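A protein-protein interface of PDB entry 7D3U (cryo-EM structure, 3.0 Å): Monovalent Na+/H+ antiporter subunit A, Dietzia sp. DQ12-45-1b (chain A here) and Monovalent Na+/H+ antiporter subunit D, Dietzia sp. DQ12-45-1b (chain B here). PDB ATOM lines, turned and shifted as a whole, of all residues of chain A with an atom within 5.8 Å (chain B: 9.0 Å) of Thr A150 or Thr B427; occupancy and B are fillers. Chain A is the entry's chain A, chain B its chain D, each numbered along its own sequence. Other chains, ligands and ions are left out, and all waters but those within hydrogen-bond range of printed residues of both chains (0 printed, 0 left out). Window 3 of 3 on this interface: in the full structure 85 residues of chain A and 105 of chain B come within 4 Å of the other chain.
The backbone carbonyl oxygen of Leu B423 is in hydrogen-bond range of the side-chain hydroxyl of Thr B427, 2.7 Å away.
O of Trp B426 is in hydrogen-bond range of N of Leu B431, at 2.9 Å.
Among the printed residues, pairs that only touch across the chains: Phe A139 with Phe B374, Phe A139 with Leu B423, Phe A139 with Trp B426, Pro A147 with Glu B433, Thr A150 with Thr B427, Thr A150 with Leu B431 and Val A154 with Thr B427.
Of chain B, only Thr B427 and Leu B431 come within 4 Å of Thr A150.
Thr B427 touches just these residues of chain A: Thr A150 (3.7 Å) and Val A154 (3.3 Å).
No residue of chain B comes within 4 Å of Gly A149.
Of the printed residues of chain A, Phe B374 touches Phe A139.
Of the printed residues of chain A, Leu B431 touches Thr A150.
Printed residues of chain A within 4 Å of Trp B426: Phe A139 (3.8 Å).
The nearest residue of chain B that does not touch Thr A150 is Gly B432 (5.6 Å).
The nearest residue of chain A that does not touch Thr B427 is Gln A151 (4.3 Å).
The nearest printed residue of chain A that does not touch Glu B433 is Gly A146 (4.6 Å).
Hydrophobic or aromatic side chains of chain A that line the printed part of chain B: Phe A139, Pro A147 and Val A154.
Of the 25 printed residues of chain B, 6 touch a printed residue of chain A.
Hydrophobic or aromatic side chains of chain B within 4 Å of the printed part of chain A: Phe B374, Leu B423, Trp B426 and Leu B431.
Among the printed residues, 7 pairs touch across the chains.
Among the printed residues, no Asp or Glu carboxylate lies within 4 Å of a Lys or Arg side-chain nitrogen of the other chain.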
ATOM      1  N   PHE A 139     -12.945  -9.583 -12.234  1.00  0.00           N
ATOM      2  CA  PHE A 139     -13.981  -9.525 -13.258  1.00  0.00           C
ATOM      3  C   PHE A 139     -14.528 -10.913 -13.553  1.00  0.00           C
ATOM      4  O   PHE A 139     -15.744 -11.112 -13.625  1.00  0.00           O
ATOM      5  CB  PHE A 139     -13.429  -8.881 -14.529  1.00  0.00           C
ATOM      6  CG  PHE A 139     -14.279  -9.115 -15.743  1.00  0.00           C
ATOM      7  CD1 PHE A 139     -15.425  -8.374 -15.956  1.00  0.00           C
ATOM      8  CD2 PHE A 139     -13.930 -10.073 -16.675  1.00  0.00           C
ATOM      9  CE1 PHE A 139     -16.207  -8.586 -17.071  1.00  0.00           C
ATOM     10  CE2 PHE A 139     -14.709 -10.288 -17.789  1.00  0.00           C
ATOM     11  CZ  PHE A 139     -15.848  -9.544 -17.987  1.00  0.00           C
ATOM     12  N   ILE A 142     -16.727 -12.190 -10.720  1.00  0.00           N
ATOM     13  CA  ILE A 142     -18.064 -11.608 -10.707  1.00  0.00           C
ATOM     14  C   ILE A 142     -18.898 -12.142 -11.867  1.00  0.00           C
ATOM     15  O   ILE A 142     -20.120 -12.291 -11.740  1.00  0.00           O
ATOM     16  CB  ILE A 142     -17.996 -10.070 -10.718  1.00  0.00           C
ATOM     17  CG1 ILE A 142     -17.061  -9.563  -9.622  1.00  0.00           C
ATOM     18  CG2 ILE A 142     -19.374  -9.476 -10.513  1.00  0.00           C
ATOM     19  CD1 ILE A 142     -17.441 -10.017  -8.239  1.00  0.00           C
ATOM     20  N   THR A 143     -18.272 -12.449 -13.009  1.00  0.00           N
ATOM     21  CA  THR A 143     -19.024 -13.031 -14.121  1.00  0.00           C
ATOM     22  C   THR A 143     -19.626 -14.386 -13.783  1.00  0.00           C
ATOM     23  O   THR A 143     -20.484 -14.864 -14.533  1.00  0.00           O
ATOM     24  CB  THR A 143     -18.158 -13.191 -15.374  1.00  0.00           C
ATOM     25  OG1 THR A 143     -17.056 -14.064 -15.098  1.00  0.00           O
ATOM     26  CG2 THR A 143     -17.665 -11.853 -15.883  1.00  0.00           C
ATOM     27  N   LEU A 144     -19.208 -15.017 -12.690  1.00  0.00           N
ATOM     28  CA  LEU A 144     -19.850 -16.241 -12.243  1.00  0.00           C
ATOM     29  C   LEU A 144     -21.247 -15.928 -11.710  1.00  0.00           C
ATOM     30  O   LEU A 144     -21.721 -14.788 -11.747  1.00  0.00           O
ATOM     31  CB  LEU A 144     -18.995 -16.939 -11.189  1.00  0.00           C
ATOM     32  CG  LEU A 144     -17.675 -17.531 -11.684  1.00  0.00           C
ATOM     33  CD1 LEU A 144     -17.112 -18.511 -10.674  1.00  0.00           C
ATOM     34  CD2 LEU A 144     -17.863 -18.202 -13.031  1.00  0.00           C
ATOM     35  N   GLY A 146     -23.995 -17.029 -13.073  1.00  0.00           N
ATOM     36  CA  GLY A 146     -24.857 -16.839 -14.215  1.00  0.00           C
ATOM     37  C   GLY A 146     -24.912 -15.408 -14.707  1.00  0.00           C
ATOM     38  O   GLY A 146     -23.969 -14.629 -14.540  1.00  0.00           O
ATOM     39  N   PRO A 147     -26.033 -15.036 -15.328  1.00  0.00           N
ATOM     40  CA  PRO A 147     -26.183 -13.678 -15.858  1.00  0.00           C
ATOM     41  C   PRO A 147     -26.600 -12.652 -14.821  1.00  0.00           C
ATOM     42  O   PRO A 147     -26.771 -11.480 -15.172  1.00  0.00           O
ATOM     43  CB  PRO A 147     -27.273 -13.842 -16.931  1.00  0.00           C
ATOM     44  CG  PRO A 147     -27.823 -15.247 -16.770  1.00  0.00           C
ATOM     45  CD  PRO A 147     -27.250 -15.834 -15.526  1.00  0.00           C
ATOM     46  N   LYS A 148     -26.787 -13.058 -13.564  1.00  0.00           N
ATOM     47  CA  LYS A 148     -27.103 -12.095 -12.517  1.00  0.00           C
ATOM     48  C   LYS A 148     -26.001 -11.056 -12.368  1.00  0.00           C
ATOM     49  O   LYS A 148     -26.278  -9.905 -12.013  1.00  0.00           O
ATOM     50  CB  LYS A 148     -27.331 -12.817 -11.191  1.00  0.00           C
ATOM     51  CG  LYS A 148     -28.791 -12.994 -10.821  1.00  0.00           C
ATOM     52  CD  LYS A 148     -29.455 -11.659 -10.535  1.00  0.00           C
ATOM     53  CE  LYS A 148     -30.841 -11.855  -9.943  1.00  0.00           C
ATOM     54  NZ  LYS A 148     -31.547 -10.564  -9.726  1.00  0.00           N
ATOM     55  N   GLY A 149     -24.757 -11.438 -12.638  1.00  0.00           N
ATOM     56  CA  GLY A 149     -23.641 -10.538 -12.452  1.00  0.00           C
ATOM     57  C   GLY A 149     -22.788 -10.321 -13.681  1.00  0.00           C
ATOM     58  O   GLY A 149     -21.561 -10.234 -13.576  1.00  0.00           O
ATOM     59  N   THR A 150     -23.412 -10.235 -14.855  1.00  0.00           N
ATOM     60  CA  THR A 150     -22.648  -9.906 -16.052  1.00  0.00           C
ATOM     61  C   THR A 150     -22.488  -8.403 -16.224  1.00  0.00           C
ATOM     62  O   THR A 150     -21.476  -7.952 -16.770  1.00  0.00           O
ATOM     63  CB  THR A 150     -23.307 -10.502 -17.294  1.00  0.00           C
ATOM     64  OG1 THR A 150     -22.700  -9.947 -18.466  1.00  0.00           O
ATOM     65  CG2 THR A 150     -24.792 -10.192 -17.313  1.00  0.00           C
ATOM     66  N   GLN A 151     -23.462  -7.620 -15.775  1.00  0.00           N
ATOM     67  CA  GLN A 151     -23.357  -6.168 -15.815  1.00  0.00           C
ATOM     68  C   GLN A 151     -22.507  -5.650 -14.656  1.00  0.00           C
ATOM     69  O   GLN A 151     -21.644  -4.788 -14.875  1.00  0.00           O
ATOM     70  CB  GLN A 151     -24.744  -5.524 -15.810  1.00  0.00           C
ATOM     71  CG  GLN A 151     -24.852  -4.309 -16.702  1.00  0.00           C
ATOM     72  CD  GLN A 151     -24.614  -4.644 -18.156  1.00  0.00           C
ATOM     73  OE1 GLN A 151     -25.117  -5.645 -18.663  1.00  0.00           O
ATOM     74  NE2 GLN A 151     -23.840  -3.810 -18.835  1.00  0.00           N
ATOM     75  N   PRO A 152     -22.717  -6.113 -13.415  1.00  0.00           N
ATOM     76  CA  PRO A 152     -21.805  -5.700 -12.338  1.00  0.00           C
ATOM     77  C   PRO A 152     -20.357  -6.041 -12.614  1.00  0.00           C
ATOM     78  O   PRO A 152     -19.472  -5.263 -12.247  1.00  0.00           O
ATOM     79  CB  PRO A 152     -22.339  -6.460 -11.119  1.00  0.00           C
ATOM     80  CG  PRO A 152     -23.773  -6.610 -11.396  1.00  0.00           C
ATOM     81  CD  PRO A 152     -23.859  -6.873 -12.869  1.00  0.00           C
ATOM     82  N   ALA A 153     -20.082  -7.173 -13.263  1.00  0.00           N
ATOM     83  CA  ALA A 153     -18.702  -7.506 -13.596  1.00  0.00           C
ATOM     84  C   ALA A 153     -18.130  -6.533 -14.617  1.00  0.00           C
ATOM     85  O   ALA A 153     -16.973  -6.114 -14.503  1.00  0.00           O
ATOM     86  CB  ALA A 153     -18.616  -8.936 -14.118  1.00  0.00           C
ATOM     87  N   VAL A 154     -18.927  -6.159 -15.621  1.00  0.00           N
ATOM     88  CA  VAL A 154     -18.465  -5.199 -16.617  1.00  0.00           C
ATOM     89  C   VAL A 154     -18.168  -3.858 -15.960  1.00  0.00           C
ATOM     90  O   VAL A 154     -17.139  -3.230 -16.234  1.00  0.00           O
ATOM     91  CB  VAL A 154     -19.499  -5.060 -17.748  1.00  0.00           C
ATOM     92  CG1 VAL A 154     -19.258  -3.787 -18.536  1.00  0.00           C
ATOM     93  CG2 VAL A 154     -19.442  -6.266 -18.664  1.00  0.00           C
ATOM     94  N   ARG A 155     -19.054  -3.407 -15.073  1.00  0.00           N
ATOM     95  CA  ARG A 155     -18.831  -2.128 -14.408  1.00  0.00           C
ATOM     96  C   ARG A 155     -17.631  -2.191 -13.474  1.00  0.00           C
ATOM     97  O   ARG A 155     -16.863  -1.229 -13.380  1.00  0.00           O
ATOM     98  CB  ARG A 155     -20.087  -1.706 -13.653  1.00  0.00           C
ATOM     99  CG  ARG A 155     -21.264  -1.457 -14.568  1.00  0.00           C
ATOM    100  CD  ARG A 155     -22.417  -0.833 -13.825  1.00  0.00           C
ATOM    101  NE  ARG A 155     -23.190  -1.824 -13.086  1.00  0.00           N
ATOM    102  CZ  ARG A 155     -24.440  -2.164 -13.380  1.00  0.00           C
ATOM    103  NH1 ARG A 155     -25.062  -1.592 -14.400  1.00  0.00           N
ATOM    104  NH2 ARG A 155     -25.069  -3.077 -12.653  1.00  0.00           N
ATOM    105  N   LEU B 356     -25.317  -7.103 -32.054  1.00  0.00           N
ATOM    106  CA  LEU B 356     -24.930  -7.455 -30.695  1.00  0.00           C
ATOM    107  C   LEU B 356     -26.190  -7.622 -29.857  1.00  0.00           C
ATOM    108  O   LEU B 356     -26.990  -6.688 -29.738  1.00  0.00           O
ATOM    109  CB  LEU B 356     -24.017  -6.390 -30.091  1.00  0.00           C
ATOM    110  CG  LEU B 356     -22.604  -6.289 -30.663  1.00  0.00           C
ATOM    111  CD1 LEU B 356     -21.726  -5.458 -29.749  1.00  0.00           C
ATOM    112  CD2 LEU B 356     -22.010  -7.665 -30.864  1.00  0.00           C
ATOM    113  N   GLY B 357     -26.364  -8.806 -29.279  1.00  0.00           N
ATOM    114  CA  GLY B 357     -27.536  -9.133 -28.500  1.00  0.00           C
ATOM    115  C   GLY B 357     -28.418 -10.191 -29.123  1.00  0.00           C
ATOM    116  O   GLY B 357     -29.222 -10.806 -28.411  1.00  0.00           O
ATOM    117  N   GLN B 358     -28.295 -10.422 -30.432  1.00  0.00           N
ATOM    118  CA  GLN B 358     -29.067 -11.480 -31.069  1.00  0.00           C
ATOM    119  C   GLN B 358     -28.545 -12.861 -30.703  1.00  0.00           C
ATOM    120  O   GLN B 358     -29.288 -13.841 -30.814  1.00  0.00           O
ATOM    121  CB  GLN B 358     -29.057 -11.299 -32.585  1.00  0.00           C
ATOM    122  CG  GLN B 358     -29.297  -9.872 -33.033  1.00  0.00           C
ATOM    123  CD  GLN B 358     -30.631  -9.334 -32.570  1.00  0.00           C
ATOM    124  OE1 GLN B 358     -30.706  -8.265 -31.967  1.00  0.00           O
ATOM    125  NE2 GLN B 358     -31.694 -10.072 -32.850  1.00  0.00           N
ATOM    126  N   LEU B 359     -27.291 -12.958 -30.279  1.00  0.00           N
ATOM    127  CA  LEU B 359     -26.714 -14.188 -29.762  1.00  0.00           C
ATOM    128  C   LEU B 359     -26.420 -14.024 -28.279  1.00  0.00           C
ATOM    129  O   LEU B 359     -26.354 -12.910 -27.756  1.00  0.00           O
ATOM    130  CB  LEU B 359     -25.432 -14.556 -30.514  1.00  0.00           C
ATOM    131  CG  LEU B 359     -25.581 -14.859 -32.003  1.00  0.00           C
ATOM    132  CD1 LEU B 359     -24.233 -14.786 -32.692  1.00  0.00           C
ATOM    133  CD2 LEU B 359     -26.213 -16.222 -32.202  1.00  0.00           C
ATOM    134  N   SER B 360     -26.238 -15.154 -27.601  1.00  0.00           N
ATOM    135  CA  SER B 360     -25.974 -15.127 -26.171  1.00  0.00           C
ATOM    136  C   SER B 360     -25.432 -16.478 -25.737  1.00  0.00           C
ATOM    137  O   SER B 360     -25.764 -17.511 -26.320  1.00  0.00           O
ATOM    138  CB  SER B 360     -27.238 -14.783 -25.375  1.00  0.00           C
ATOM    139  OG  SER B 360     -27.675 -13.466 -25.660  1.00  0.00           O
ATOM    140  N   GLY B 361     -24.593 -16.453 -24.706  1.00  0.00           N
ATOM    141  CA  GLY B 361     -24.094 -17.679 -24.122  1.00  0.00           C
ATOM    142  C   GLY B 361     -23.037 -18.397 -24.923  1.00  0.00           C
ATOM    143  O   GLY B 361     -22.711 -19.542 -24.595  1.00  0.00           O
ATOM    144  N   LEU B 362     -22.487 -17.768 -25.963  1.00  0.00           N
ATOM    145  CA  LEU B 362     -21.467 -18.424 -26.769  1.00  0.00           C
ATOM    146  C   LEU B 362     -20.212 -18.742 -25.970  1.00  0.00           C
ATOM    147  O   LEU B 362     -19.403 -19.566 -26.409  1.00  0.00           O
ATOM    148  CB  LEU B 362     -21.109 -17.558 -27.975  1.00  0.00           C
ATOM    149  CG  LEU B 362     -21.775 -17.962 -29.287  1.00  0.00           C
ATOM    150  CD1 LEU B 362     -23.277 -18.048 -29.116  1.00  0.00           C
ATOM    151  CD2 LEU B 362     -21.420 -16.982 -30.381  1.00  0.00           C
ATOM    152  N   ALA B 363     -20.026 -18.110 -24.810  1.00  0.00           N
ATOM    153  CA  ALA B 363     -18.914 -18.472 -23.943  1.00  0.00           C
ATOM    154  C   ALA B 363     -19.148 -19.798 -23.241  1.00  0.00           C
ATOM    155  O   ALA B 363     -18.192 -20.395 -22.736  1.00  0.00           O
ATOM    156  CB  ALA B 363     -18.670 -17.374 -22.910  1.00  0.00           C
ATOM    157  N   PHE B 373     -11.088 -15.266 -28.306  1.00  0.00           N
ATOM    158  CA  PHE B 373     -11.519 -13.884 -28.448  1.00  0.00           C
ATOM    159  C   PHE B 373     -11.151 -13.053 -27.231  1.00  0.00           C
ATOM    160  O   PHE B 373     -10.727 -11.907 -27.377  1.00  0.00           O
ATOM    161  CB  PHE B 373     -13.025 -13.806 -28.687  1.00  0.00           C
ATOM    162  CG  PHE B 373     -13.583 -12.421 -28.534  1.00  0.00           C
ATOM    163  CD1 PHE B 373     -13.581 -11.541 -29.598  1.00  0.00           C
ATOM    164  CD2 PHE B 373     -14.109 -11.996 -27.326  1.00  0.00           C
ATOM    165  CE1 PHE B 373     -14.085 -10.268 -29.459  1.00  0.00           C
ATOM    166  CE2 PHE B 373     -14.611 -10.724 -27.184  1.00  0.00           C
ATOM    167  CZ  PHE B 373     -14.599  -9.861 -28.251  1.00  0.00           C
ATOM    168  N   PHE B 374     -11.329 -13.592 -26.024  1.00  0.00           N
ATOM    169  CA  PHE B 374     -11.075 -12.781 -24.839  1.00  0.00           C
ATOM    170  C   PHE B 374      -9.589 -12.512 -24.664  1.00  0.00           C
ATOM    171  O   PHE B 374      -9.199 -11.420 -24.234  1.00  0.00           O
ATOM    172  CB  PHE B 374     -11.639 -13.446 -23.590  1.00  0.00           C
ATOM    173  CG  PHE B 374     -11.808 -12.501 -22.440  1.00  0.00           C
ATOM    174  CD1 PHE B 374     -12.903 -11.661 -22.375  1.00  0.00           C
ATOM    175  CD2 PHE B 374     -10.857 -12.427 -21.442  1.00  0.00           C
ATOM    176  CE1 PHE B 374     -13.058 -10.783 -21.327  1.00  0.00           C
ATOM    177  CE2 PHE B 374     -11.007 -11.548 -20.393  1.00  0.00           C
ATOM    178  CZ  PHE B 374     -12.110 -10.728 -20.334  1.00  0.00           C
ATOM    179  N   LEU B 419     -11.527  -0.966 -24.188  1.00  0.00           N
ATOM    180  CA  LEU B 419     -12.007  -1.995 -23.278  1.00  0.00           C
ATOM    181  C   LEU B 419     -13.522  -1.960 -23.162  1.00  0.00           C
ATOM    182  O   LEU B 419     -14.166  -3.010 -23.080  1.00  0.00           O
ATOM    183  CB  LEU B 419     -11.363  -1.827 -21.905  1.00  0.00           C
ATOM    184  CG  LEU B 419     -11.749  -2.907 -20.898  1.00  0.00           C
ATOM    185  CD1 LEU B 419     -11.404  -4.274 -21.450  1.00  0.00           C
ATOM    186  CD2 LEU B 419     -11.065  -2.675 -19.568  1.00  0.00           C
ATOM    187  N   LEU B 420     -14.113  -0.763 -23.156  1.00  0.00           N
ATOM    188  CA  LEU B 420     -15.566  -0.657 -23.099  1.00  0.00           C
ATOM    189  C   LEU B 420     -16.214  -1.340 -24.294  1.00  0.00           C
ATOM    190  O   LEU B 420     -17.193  -2.076 -24.142  1.00  0.00           O
ATOM    191  CB  LEU B 420     -15.979   0.814 -23.033  1.00  0.00           C
ATOM    192  CG  LEU B 420     -17.460   1.156 -23.214  1.00  0.00           C
ATOM    193  CD1 LEU B 420     -18.328   0.349 -22.267  1.00  0.00           C
ATOM    194  CD2 LEU B 420     -17.685   2.641 -23.004  1.00  0.00           C
ATOM    195  N   SER B 421     -15.666  -1.133 -25.489  1.00  0.00           N
ATOM    196  CA  SER B 421     -16.279  -1.724 -26.675  1.00  0.00           C
ATOM    197  C   SER B 421     -16.030  -3.227 -26.740  1.00  0.00           C
ATOM    198  O   SER B 421     -16.923  -3.995 -27.128  1.00  0.00           O
ATOM    199  CB  SER B 421     -15.765  -1.032 -27.931  1.00  0.00           C
ATOM    200  OG  SER B 421     -15.882  -1.888 -29.048  1.00  0.00           O
ATOM    201  N   MET B 422     -14.831  -3.672 -26.362  1.00  0.00           N
ATOM    202  CA  MET B 422     -14.582  -5.109 -26.328  1.00  0.00           C
ATOM    203  C   MET B 422     -15.461  -5.795 -25.292  1.00  0.00           C
ATOM    204  O   MET B 422     -15.923  -6.919 -25.515  1.00  0.00           O
ATOM    205  CB  MET B 422     -13.106  -5.393 -26.050  1.00  0.00           C
ATOM    206  CG  MET B 422     -12.158  -4.872 -27.117  1.00  0.00           C
ATOM    207  SD  MET B 422     -12.733  -5.178 -28.795  1.00  0.00           S
ATOM    208  CE  MET B 422     -12.593  -6.956 -28.883  1.00  0.00           C
ATOM    209  N   LEU B 423     -15.733  -5.126 -24.170  1.00  0.00           N
ATOM    210  CA  LEU B 423     -16.652  -5.677 -23.184  1.00  0.00           C
ATOM    211  C   LEU B 423     -18.084  -5.654 -23.690  1.00  0.00           C
ATOM    212  O   LEU B 423     -18.866  -6.545 -23.355  1.00  0.00           O
ATOM    213  CB  LEU B 423     -16.547  -4.902 -21.874  1.00  0.00           C
ATOM    214  CG  LEU B 423     -15.346  -5.238 -20.995  1.00  0.00           C
ATOM    215  CD1 LEU B 423     -15.425  -4.475 -19.689  1.00  0.00           C
ATOM    216  CD2 LEU B 423     -15.271  -6.731 -20.745  1.00  0.00           C
ATOM    217  N   LYS B 424     -18.444  -4.652 -24.492  1.00  0.00           N
ATOM    218  CA  LYS B 424     -19.760  -4.657 -25.118  1.00  0.00           C
ATOM    219  C   LYS B 424     -19.923  -5.869 -26.022  1.00  0.00           C
ATOM    220  O   LYS B 424     -20.971  -6.525 -26.010  1.00  0.00           O
ATOM    221  CB  LYS B 424     -19.973  -3.368 -25.906  1.00  0.00           C
ATOM    222  CG  LYS B 424     -21.430  -3.019 -26.128  1.00  0.00           C
ATOM    223  CD  LYS B 424     -21.639  -1.519 -26.115  1.00  0.00           C
ATOM    224  CE  LYS B 424     -20.660  -0.817 -27.038  1.00  0.00           C
ATOM    225  NZ  LYS B 424     -20.753  -1.317 -28.437  1.00  0.00           N
ATOM    226  N   ILE B 425     -18.889  -6.195 -26.799  1.00  0.00           N
ATOM    227  CA  ILE B 425     -18.946  -7.394 -27.635  1.00  0.00           C
ATOM    228  C   ILE B 425     -19.044  -8.642 -26.765  1.00  0.00           C
ATOM    229  O   ILE B 425     -19.897  -9.513 -26.981  1.00  0.00           O
ATOM    230  CB  ILE B 425     -17.729  -7.465 -28.571  1.00  0.00           C
ATOM    231  CG1 ILE B 425     -17.767  -6.338 -29.594  1.00  0.00           C
ATOM    232  CG2 ILE B 425     -17.708  -8.792 -29.295  1.00  0.00           C
ATOM    233  CD1 ILE B 425     -16.625  -6.387 -30.572  1.00  0.00           C
ATOM    234  N   TRP B 426     -18.159  -8.746 -25.770  1.00  0.00           N
ATOM    235  CA  TRP B 426     -18.125  -9.908 -24.888  1.00  0.00           C
ATOM    236  C   TRP B 426     -19.447 -10.106 -24.158  1.00  0.00           C
ATOM    237  O   TRP B 426     -19.826 -11.243 -23.860  1.00  0.00           O
ATOM    238  CB  TRP B 426     -16.973  -9.743 -23.893  1.00  0.00           C
ATOM    239  CG  TRP B 426     -16.866 -10.794 -22.838  1.00  0.00           C
ATOM    240  CD1 TRP B 426     -17.209 -10.668 -21.525  1.00  0.00           C
ATOM    241  CD2 TRP B 426     -16.346 -12.119 -22.990  1.00  0.00           C
ATOM    242  NE1 TRP B 426     -16.952 -11.837 -20.854  1.00  0.00           N
ATOM    243  CE2 TRP B 426     -16.422 -12.743 -21.733  1.00  0.00           C
ATOM    244  CE3 TRP B 426     -15.835 -12.840 -24.070  1.00  0.00           C
ATOM    245  CZ2 TRP B 426     -16.005 -14.053 -21.525  1.00  0.00           C
ATOM    246  CZ3 TRP B 426     -15.420 -14.139 -23.862  1.00  0.00           C
ATOM    247  CH2 TRP B 426     -15.507 -14.733 -22.601  1.00  0.00           C
ATOM    248  N   THR B 427     -20.163  -9.020 -23.871  1.00  0.00           N
ATOM    249  CA  THR B 427     -21.429  -9.115 -23.157  1.00  0.00           C
ATOM    250  C   THR B 427     -22.585  -9.407 -24.104  1.00  0.00           C
ATOM    251  O   THR B 427     -23.512 -10.142 -23.747  1.00  0.00           O
ATOM    252  CB  THR B 427     -21.687  -7.820 -22.388  1.00  0.00           C
ATOM    253  OG1 THR B 427     -20.586  -7.562 -21.510  1.00  0.00           O
ATOM    254  CG2 THR B 427     -22.959  -7.925 -21.570  1.00  0.00           C
ATOM    255  N   GLY B 428     -22.548  -8.851 -25.313  1.00  0.00           N
ATOM    256  CA  GLY B 428     -23.631  -9.054 -26.251  1.00  0.00           C
ATOM    257  C   GLY B 428     -23.551 -10.321 -27.066  1.00  0.00           C
ATOM    258  O   GLY B 428     -24.527 -10.665 -27.737  1.00  0.00           O
ATOM    259  N   ILE B 429     -22.422 -11.027 -27.033  1.00  0.00           N
ATOM    260  CA  ILE B 429     -22.248 -12.263 -27.783  1.00  0.00           C
ATOM    261  C   ILE B 429     -21.975 -13.448 -26.864  1.00  0.00           C
ATOM    262  O   ILE B 429     -22.580 -14.514 -27.010  1.00  0.00           O
ATOM    263  CB  ILE B 429     -21.132 -12.128 -28.842  1.00  0.00           C
ATOM    264  CG1 ILE B 429     -21.577 -11.197 -29.966  1.00  0.00           C
ATOM    265  CG2 ILE B 429     -20.762 -13.483 -29.407  1.00  0.00           C
ATOM    266  CD1 ILE B 429     -20.607 -11.137 -31.116  1.00  0.00           C
ATOM    267  N   PHE B 430     -21.073 -13.277 -25.900  1.00  0.00           N
ATOM    268  CA  PHE B 430     -20.558 -14.416 -25.150  1.00  0.00           C
ATOM    269  C   PHE B 430     -21.196 -14.599 -23.782  1.00  0.00           C
ATOM    270  O   PHE B 430     -21.416 -15.740 -23.368  1.00  0.00           O
ATOM    271  CB  PHE B 430     -19.042 -14.290 -24.981  1.00  0.00           C
ATOM    272  CG  PHE B 430     -18.283 -14.405 -26.269  1.00  0.00           C
ATOM    273  CD1 PHE B 430     -18.010 -13.284 -27.028  1.00  0.00           C
ATOM    274  CD2 PHE B 430     -17.857 -15.635 -26.728  1.00  0.00           C
ATOM    275  CE1 PHE B 430     -17.318 -13.388 -28.212  1.00  0.00           C
ATOM    276  CE2 PHE B 430     -17.165 -15.741 -27.914  1.00  0.00           C
ATOM    277  CZ  PHE B 430     -16.895 -14.617 -28.654  1.00  0.00           C
ATOM    278  N   LEU B 431     -21.504 -13.522 -23.069  1.00  0.00           N
ATOM    279  CA  LEU B 431     -22.069 -13.631 -21.732  1.00  0.00           C
ATOM    280  C   LEU B 431     -23.590 -13.678 -21.804  1.00  0.00           C
ATOM    281  O   LEU B 431     -24.213 -12.863 -22.491  1.00  0.00           O
ATOM    282  CB  LEU B 431     -21.617 -12.465 -20.855  1.00  0.00           C
ATOM    283  CG  LEU B 431     -20.164 -12.518 -20.387  1.00  0.00           C
ATOM    284  CD1 LEU B 431     -19.905 -11.446 -19.344  1.00  0.00           C
ATOM    285  CD2 LEU B 431     -19.828 -13.892 -19.841  1.00  0.00           C
ATOM    286  N   GLY B 432     -24.179 -14.633 -21.091  1.00  0.00           N
ATOM    287  CA  GLY B 432     -25.620 -14.774 -21.058  1.00  0.00           C
ATOM    288  C   GLY B 432     -26.061 -16.221 -21.067  1.00  0.00           C
ATOM    289  O   GLY B 432     -25.227 -17.129 -21.121  1.00  0.00           O
ATOM    290  N   GLU B 433     -27.369 -16.452 -21.009  1.00  0.00           N
ATOM    291  CA  GLU B 433     -27.763 -17.853 -21.086  1.00  0.00           C
ATOM    292  C   GLU B 433     -27.921 -18.275 -22.543  1.00  0.00           C
ATOM    293  O   GLU B 433     -28.468 -17.521 -23.352  1.00  0.00           O
ATOM    294  CB  GLU B 433     -29.075 -18.087 -20.347  1.00  0.00           C
ATOM    295  CG  GLU B 433     -28.950 -18.055 -18.838  1.00  0.00           C
ATOM    296  CD  GLU B 433     -28.174 -19.234 -18.294  1.00  0.00           C
ATOM    297  OE1 GLU B 433     -28.151 -20.292 -18.958  1.00  0.00           O
ATOM    298  OE2 GLU B 433     -27.584 -19.104 -17.202  1.00  0.00           O
